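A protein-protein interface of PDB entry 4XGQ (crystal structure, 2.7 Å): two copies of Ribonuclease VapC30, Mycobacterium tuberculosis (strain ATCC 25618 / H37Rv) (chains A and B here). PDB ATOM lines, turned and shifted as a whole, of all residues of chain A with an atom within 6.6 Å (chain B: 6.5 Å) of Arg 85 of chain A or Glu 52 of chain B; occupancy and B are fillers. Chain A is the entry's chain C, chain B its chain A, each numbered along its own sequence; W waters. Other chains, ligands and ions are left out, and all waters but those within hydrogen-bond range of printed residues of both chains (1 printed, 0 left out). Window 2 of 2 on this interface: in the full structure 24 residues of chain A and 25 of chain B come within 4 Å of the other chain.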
ATOM      1  N   ASP A  78     -19.604  20.235 -36.034  1.00  0.00           N
ATOM      2  CA  ASP A  78     -19.174  19.134 -35.167  1.00  0.00           C
ATOM      3  C   ASP A  78     -18.507  19.667 -33.904  1.00  0.00           C
ATOM      4  O   ASP A  78     -18.712  19.143 -32.811  1.00  0.00           O
ATOM      5  CB  ASP A  78     -18.241  18.171 -35.910  1.00  0.00           C
ATOM      6  CG  ASP A  78     -18.983  17.325 -36.958  1.00  0.00           C
ATOM      7  OD1 ASP A  78     -20.242  17.222 -36.882  1.00  0.00           O
ATOM      8  OD2 ASP A  78     -18.298  16.758 -37.867  1.00  0.00           O
ATOM      9  N   ALA A  80     -18.925  22.575 -32.546  1.00  0.00           N
ATOM     10  CA  ALA A  80     -19.928  23.216 -31.749  1.00  0.00           C
ATOM     11  C   ALA A  80     -20.791  22.192 -31.001  1.00  0.00           C
ATOM     12  O   ALA A  80     -21.199  22.404 -29.822  1.00  0.00           O
ATOM     13  CB  ALA A  80     -20.789  24.079 -32.659  1.00  0.00           C
ATOM     14  N   ARG A  81     -21.110  21.112 -31.721  1.00  0.00           N
ATOM     15  CA  ARG A  81     -21.883  20.011 -31.179  1.00  0.00           C
ATOM     16  C   ARG A  81     -21.282  19.493 -29.884  1.00  0.00           C
ATOM     17  O   ARG A  81     -21.986  19.309 -28.927  1.00  0.00           O
ATOM     18  CB  ARG A  81     -21.934  18.873 -32.201  1.00  0.00           C
ATOM     19  CG  ARG A  81     -22.626  17.596 -31.732  1.00  0.00           C
ATOM     20  CD  ARG A  81     -22.803  16.637 -32.901  1.00  0.00           C
ATOM     21  NE  ARG A  81     -23.313  15.352 -32.427  1.00  0.00           N
ATOM     22  CZ  ARG A  81     -23.609  14.315 -33.204  1.00  0.00           C
ATOM     23  NH1 ARG A  81     -23.471  14.378 -34.526  1.00  0.00           N
ATOM     24  NH2 ARG A  81     -24.059  13.199 -32.651  1.00  0.00           N
ATOM     25  N   ALA A  82     -19.972  19.284 -29.858  1.00  0.00           N
ATOM     26  CA  ALA A  82     -19.259  18.864 -28.657  1.00  0.00           C
ATOM     27  C   ALA A  82     -19.221  19.976 -27.624  1.00  0.00           C
ATOM     28  O   ALA A  82     -19.482  19.755 -26.444  1.00  0.00           O
ATOM     29  CB  ALA A  82     -17.853  18.435 -29.027  1.00  0.00           C
ATOM     30  N   ALA A  83     -18.928  21.186 -28.061  1.00  0.00           N
ATOM     31  CA  ALA A  83     -18.781  22.294 -27.113  1.00  0.00           C
ATOM     32  C   ALA A  83     -20.036  22.566 -26.311  1.00  0.00           C
ATOM     33  O   ALA A  83     -19.965  22.920 -25.127  1.00  0.00           O
ATOM     34  CB  ALA A  83     -18.334  23.572 -27.821  1.00  0.00           C
ATOM     35  N   TYR A  84     -21.185  22.404 -26.935  1.00  0.00           N
ATOM     36  CA  TYR A  84     -22.436  22.673 -26.235  1.00  0.00           C
ATOM     37  C   TYR A  84     -22.677  21.731 -25.021  1.00  0.00           C
ATOM     38  O   TYR A  84     -23.335  22.120 -24.066  1.00  0.00           O
ATOM     39  CB  TYR A  84     -23.608  22.604 -27.220  1.00  0.00           C
ATOM     40  CG  TYR A  84     -24.908  23.165 -26.680  1.00  0.00           C
ATOM     41  CD1 TYR A  84     -25.182  24.546 -26.718  1.00  0.00           C
ATOM     42  CD2 TYR A  84     -25.885  22.322 -26.148  1.00  0.00           C
ATOM     43  CE1 TYR A  84     -26.383  25.065 -26.223  1.00  0.00           C
ATOM     44  CE2 TYR A  84     -27.089  22.829 -25.660  1.00  0.00           C
ATOM     45  CZ  TYR A  84     -27.332  24.195 -25.688  1.00  0.00           C
ATOM     46  OH  TYR A  84     -28.530  24.651 -25.193  1.00  0.00           O
ATOM     47  N   ARG A  85     -22.146  20.507 -25.066  1.00  0.00           N
ATOM     48  CA  ARG A  85     -22.281  19.536 -23.936  1.00  0.00           C
ATOM     49  C   ARG A  85     -21.553  20.058 -22.715  1.00  0.00           C
ATOM     50  O   ARG A  85     -22.076  20.036 -21.614  1.00  0.00           O
ATOM     51  CB  ARG A  85     -21.740  18.139 -24.316  1.00  0.00           C
ATOM     52  CG  ARG A  85     -22.420  17.541 -25.558  1.00  0.00           C
ATOM     53  CD  ARG A  85     -22.238  16.057 -25.691  1.00  0.00           C
ATOM     54  NE  ARG A  85     -20.934  15.725 -26.226  1.00  0.00           N
ATOM     55  CZ  ARG A  85     -20.662  15.512 -27.517  1.00  0.00           C
ATOM     56  NH1 ARG A  85     -21.594  15.615 -28.459  1.00  0.00           N
ATOM     57  NH2 ARG A  85     -19.423  15.196 -27.890  1.00  0.00           N
ATOM     58  N   THR A  86     -20.340  20.552 -22.937  1.00  0.00           N
ATOM     59  CA  THR A  86     -19.507  21.100 -21.883  1.00  0.00           C
ATOM     60  C   THR A  86     -19.964  22.495 -21.444  1.00  0.00           C
ATOM     61  O   THR A  86     -20.154  22.762 -20.244  1.00  0.00           O
ATOM     62  CB  THR A  86     -18.067  21.219 -22.369  1.00  0.00           C
ATOM     63  OG1 THR A  86     -17.685  20.007 -23.043  1.00  0.00           O
ATOM     64  CG2 THR A  86     -17.169  21.455 -21.218  1.00  0.00           C
ATOM     65  N   TYR A  87     -20.126  23.385 -22.424  1.00  0.00           N
ATOM     66  CA  TYR A  87     -20.240  24.828 -22.145  1.00  0.00           C
ATOM     67  C   TYR A  87     -21.654  25.421 -22.320  1.00  0.00           C
ATOM     68  O   TYR A  87     -21.889  26.552 -21.903  1.00  0.00           O
ATOM     69  CB  TYR A  87     -19.244  25.595 -23.034  1.00  0.00           C
ATOM     70  CG  TYR A  87     -17.807  25.174 -22.844  1.00  0.00           C
ATOM     71  CD1 TYR A  87     -17.260  25.055 -21.567  1.00  0.00           C
ATOM     72  CD2 TYR A  87     -16.981  24.937 -23.934  1.00  0.00           C
ATOM     73  CE1 TYR A  87     -15.953  24.685 -21.371  1.00  0.00           C
ATOM     74  CE2 TYR A  87     -15.656  24.573 -23.755  1.00  0.00           C
ATOM     75  CZ  TYR A  87     -15.148  24.437 -22.469  1.00  0.00           C
ATOM     76  OH  TYR A  87     -13.832  24.038 -22.263  1.00  0.00           O
ATOM     77  N   GLY A  88     -22.578  24.668 -22.920  1.00  0.00           N
ATOM     78  CA  GLY A  88     -23.908  25.170 -23.243  1.00  0.00           C
ATOM     79  C   GLY A  88     -24.727  25.591 -22.049  1.00  0.00           C
ATOM     80  O   GLY A  88     -24.469  25.188 -20.920  1.00  0.00           O
ATOM     81  N   ARG A  93     -26.417  28.061 -15.733  1.00  0.00           N
ATOM     82  CA  ARG A  93     -25.035  27.809 -16.140  1.00  0.00           C
ATOM     83  C   ARG A  93     -24.479  28.921 -17.031  1.00  0.00           C
ATOM     84  O   ARG A  93     -23.268  29.017 -17.211  1.00  0.00           O
ATOM     85  CB  ARG A  93     -24.910  26.440 -16.815  1.00  0.00           C
ATOM     86  CG  ARG A  93     -24.884  25.289 -15.820  1.00  0.00           C
ATOM     87  CD  ARG A  93     -25.211  23.954 -16.466  1.00  0.00           C
ATOM     88  NE  ARG A  93     -24.656  23.830 -17.812  1.00  0.00           N
ATOM     89  CZ  ARG A  93     -23.362  23.704 -18.095  1.00  0.00           C
ATOM     90  NH1 ARG A  93     -22.970  23.584 -19.357  1.00  0.00           N
ATOM     91  NH2 ARG A  93     -22.454  23.701 -17.131  1.00  0.00           N
ATOM     92  N   LEU B  44     -28.047  19.139 -31.023  1.00  0.00           N
ATOM     93  CA  LEU B  44     -28.221  19.771 -29.706  1.00  0.00           C
ATOM     94  C   LEU B  44     -29.476  19.240 -29.008  1.00  0.00           C
ATOM     95  O   LEU B  44     -29.442  18.916 -27.834  1.00  0.00           O
ATOM     96  CB  LEU B  44     -28.313  21.319 -29.823  1.00  0.00           C
ATOM     97  CG  LEU B  44     -27.195  22.090 -30.536  1.00  0.00           C
ATOM     98  CD1 LEU B  44     -27.533  23.575 -30.629  1.00  0.00           C
ATOM     99  CD2 LEU B  44     -25.862  21.892 -29.835  1.00  0.00           C
ATOM    100  N   ILE B  46     -31.496  16.546 -29.608  1.00  0.00           N
ATOM    101  CA  ILE B  46     -31.369  15.125 -29.336  1.00  0.00           C
ATOM    102  C   ILE B  46     -30.417  14.855 -28.184  1.00  0.00           C
ATOM    103  O   ILE B  46     -30.813  14.246 -27.202  1.00  0.00           O
ATOM    104  CB  ILE B  46     -30.900  14.355 -30.581  1.00  0.00           C
ATOM    105  CG1 ILE B  46     -31.975  14.379 -31.654  1.00  0.00           C
ATOM    106  CG2 ILE B  46     -30.562  12.929 -30.239  1.00  0.00           C
ATOM    107  CD1 ILE B  46     -33.296  13.787 -31.203  1.00  0.00           C
ATOM    108  N   GLU B  47     -29.180  15.326 -28.285  1.00  0.00           N
ATOM    109  CA  GLU B  47     -28.173  15.022 -27.251  1.00  0.00           C
ATOM    110  C   GLU B  47     -28.486  15.657 -25.897  1.00  0.00           C
ATOM    111  O   GLU B  47     -27.987  15.217 -24.884  1.00  0.00           O
ATOM    112  CB  GLU B  47     -26.750  15.406 -27.698  1.00  0.00           C
ATOM    113  CG  GLU B  47     -26.202  14.512 -28.793  1.00  0.00           C
ATOM    114  CD  GLU B  47     -24.740  14.775 -29.100  1.00  0.00           C
ATOM    115  OE1 GLU B  47     -24.127  15.598 -28.399  1.00  0.00           O
ATOM    116  OE2 GLU B  47     -24.206  14.190 -30.067  1.00  0.00           O
ATOM    117  N   ALA B  48     -29.292  16.702 -25.877  1.00  0.00           N
ATOM    118  CA  ALA B  48     -29.781  17.230 -24.620  1.00  0.00           C
ATOM    119  C   ALA B  48     -30.739  16.205 -24.036  1.00  0.00           C
ATOM    120  O   ALA B  48     -30.624  15.850 -22.884  1.00  0.00           O
ATOM    121  CB  ALA B  48     -30.489  18.559 -24.822  1.00  0.00           C
ATOM    122  N   PHE B  50     -31.615  12.821 -24.919  1.00  0.00           N
ATOM    123  CA  PHE B  50     -31.228  11.423 -24.816  1.00  0.00           C
ATOM    124  C   PHE B  50     -29.729  11.225 -24.616  1.00  0.00           C
ATOM    125  O   PHE B  50     -29.213  10.112 -24.804  1.00  0.00           O
ATOM    126  CB  PHE B  50     -31.635  10.698 -26.096  1.00  0.00           C
ATOM    127  CG  PHE B  50     -33.096  10.792 -26.395  1.00  0.00           C
ATOM    128  CD1 PHE B  50     -34.032  10.234 -25.523  1.00  0.00           C
ATOM    129  CD2 PHE B  50     -33.541  11.413 -27.549  1.00  0.00           C
ATOM    130  CE1 PHE B  50     -35.386  10.317 -25.794  1.00  0.00           C
ATOM    131  CE2 PHE B  50     -34.895  11.497 -27.826  1.00  0.00           C
ATOM    132  CZ  PHE B  50     -35.818  10.950 -26.946  1.00  0.00           C
ATOM    133  N   GLY B  51     -29.044  12.298 -24.223  1.00  0.00           N
ATOM    134  CA  GLY B  51     -27.606  12.269 -23.982  1.00  0.00           C
ATOM    135  C   GLY B  51     -26.811  11.995 -25.247  1.00  0.00           C
ATOM    136  O   GLY B  51     -27.362  11.953 -26.359  1.00  0.00           O
ATOM    137  N   GLU B  52     -25.520  11.753 -25.064  1.00  0.00           N
ATOM    138  CA  GLU B  52     -24.656  11.417 -26.170  1.00  0.00           C
ATOM    139  C   GLU B  52     -25.092  10.198 -26.948  1.00  0.00           C
ATOM    140  O   GLU B  52     -24.819  10.142 -28.140  1.00  0.00           O
ATOM    141  CB  GLU B  52     -23.220  11.220 -25.695  1.00  0.00           C
ATOM    142  CG  GLU B  52     -22.336  12.450 -25.873  1.00  0.00           C
ATOM    143  CD  GLU B  52     -21.058  12.350 -25.063  1.00  0.00           C
ATOM    144  OE1 GLU B  52     -20.139  11.630 -25.518  1.00  0.00           O
ATOM    145  OE2 GLU B  52     -20.974  12.976 -23.970  1.00  0.00           O
ATOM    146  N   PRO B  53     -25.741   9.206 -26.295  1.00  0.00           N
ATOM    147  CA  PRO B  53     -26.114   8.052 -27.117  1.00  0.00           C
ATOM    148  C   PRO B  53     -27.202   8.359 -28.124  1.00  0.00           C
ATOM    149  O   PRO B  53     -27.283   7.714 -29.136  1.00  0.00           O
ATOM    150  CB  PRO B  53     -26.640   7.043 -26.096  1.00  0.00           C
ATOM    151  CG  PRO B  53     -25.917   7.372 -24.852  1.00  0.00           C
ATOM    152  CD  PRO B  53     -25.855   8.878 -24.859  1.00  0.00           C
ATOM    153  N   GLY B  54     -28.063   9.304 -27.817  1.00  0.00           N
ATOM    154  CA  GLY B  54     -29.029   9.803 -28.801  1.00  0.00           C
ATOM    155  C   GLY B  54     -28.316  10.362 -30.021  1.00  0.00           C
ATOM    156  O   GLY B  54     -28.735  10.160 -31.171  1.00  0.00           O
ATOM    157  N   GLY B  55     -27.202  11.038 -29.774  1.00  0.00           N
ATOM    158  CA  GLY B  55     -26.390  11.542 -30.855  1.00  0.00           C
ATOM    159  C   GLY B  55     -25.836  10.469 -31.757  1.00  0.00           C
ATOM    160  O   GLY B  55     -25.674  10.690 -32.978  1.00  0.00           O
ATOM    161  N   ARG B  56     -25.520   9.318 -31.174  1.00  0.00           N
ATOM    162  CA  ARG B  56     -25.037   8.178 -31.974  1.00  0.00           C
ATOM    163  C   ARG B  56     -26.151   7.690 -32.912  1.00  0.00           C
ATOM    164  O   ARG B  56     -25.920   7.342 -34.096  1.00  0.00           O
ATOM    165  CB  ARG B  56     -24.532   7.054 -31.064  1.00  0.00           C
ATOM    166  CG  ARG B  56     -23.174   7.359 -30.410  1.00  0.00           C
ATOM    167  CD  ARG B  56     -22.457   6.139 -29.790  1.00  0.00           C
ATOM    168  NE  ARG B  56     -22.882   5.898 -28.392  1.00  0.00           N
ATOM    169  CZ  ARG B  56     -22.452   6.591 -27.328  1.00  0.00           C
ATOM    170  NH1 ARG B  56     -21.551   7.575 -27.465  1.00  0.00           N
ATOM    171  NH2 ARG B  56     -22.926   6.304 -26.117  1.00  0.00           N
ATOM    172  N   GLU B  57     -27.389   7.716 -32.415  1.00  0.00           N
ATOM    173  CA  GLU B  57     -28.517   7.353 -33.283  1.00  0.00           C
ATOM    174  C   GLU B  57     -28.744   8.386 -34.377  1.00  0.00           C
ATOM    175  O   GLU B  57     -29.030   8.034 -35.525  1.00  0.00           O
ATOM    176  CB  GLU B  57     -29.801   7.087 -32.482  1.00  0.00           C
ATOM    177  CG  GLU B  57     -29.699   5.954 -31.438  1.00  0.00           C
ATOM    178  CD  GLU B  57     -29.287   4.606 -32.028  1.00  0.00           C
ATOM    179  OE1 GLU B  57     -29.574   4.355 -33.215  1.00  0.00           O
ATOM    180  OE2 GLU B  57     -28.660   3.790 -31.305  1.00  0.00           O
HETATM  181  O   HOH W   1     -24.696  18.369 -28.546  1.00  0.00           O
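Among the printed residues, merely in contact across the chains: Tyr 84 of chain A with Leu 44 of chain B (3.5 Å).
Hydrophobic or aromatic side chains of chain A within 4 Å of the printed part of chain B: Tyr 84.
Printed residues of chain B that touch a printed residue of chain A: Leu 44, Glu 47, Glu 52 and Gly 55.
Hydrophobic or aromatic side chains of chain B that line the printed part of chain A: Leu 44.
The side-chain carboxylate (OE2) of Glu 47 of chain B is in salt-bridge range of the guanidinium group (NH2) of Arg 81 of chain A, 2.8 Å away.
The guanidinium group (NH1) of Arg 85 of chain A is in salt-bridge range of the side-chain carboxylate (OE1) of Glu 47 of chain B (2.5 Å).
OE2 of Glu 52 of chain B lies within salt-bridge range of NE of Arg 85 of chain A, 3.6 Å away.
O of Gly 55 of chain B lies within hydrogen-bond range of NH2 of Arg 81 of chain A, at 3.0 Å.
No position is printed for both chains.
Of the 5 pairs that touch across the chains among the printed residues, none has its exchanged pair printed and touching as well.
Water W1 bridges the side-chain carboxylate of Glu 47 of chain B and the backbone carbonyl oxygen of Arg 81 of chain A.
Printed residues of chain B within 4 Å of Arg 81 of chain A: Glu 47 (2.8 Å) and Gly 55 (3.0 Å).
Ala 83 of chain A touches none of the printed residues of chain B.
Of the printed residues of chain B, Tyr 84 of chain A touches Leu 44.
Arg 85 of chain A touches just these residues of chain B: Glu 47 (2.5 Å) and Glu 52 (3.6 Å).
Printed residues of chain A within 4 Å of Leu 44 of chain B: Tyr 84.
Of the printed residues of chain A, Glu 47 of chain B touches Arg 81 (2.8 Å) and Arg 85 (2.5 Å).
Glu 57 of chain B touches none of the printed residues of chain A.
The nearest residue of chain B that does not touch Arg 85 of chain A is Gly 51 of chain B (6.1 Å).
The nearest residue of chain A that does not touch Glu 52 of chain B is Arg 81 of chain A (5.5 Å).
The nearest printed residue of chain B that does not touch Arg 81 of chain A is Arg 56 of chain B (4.4 Å).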
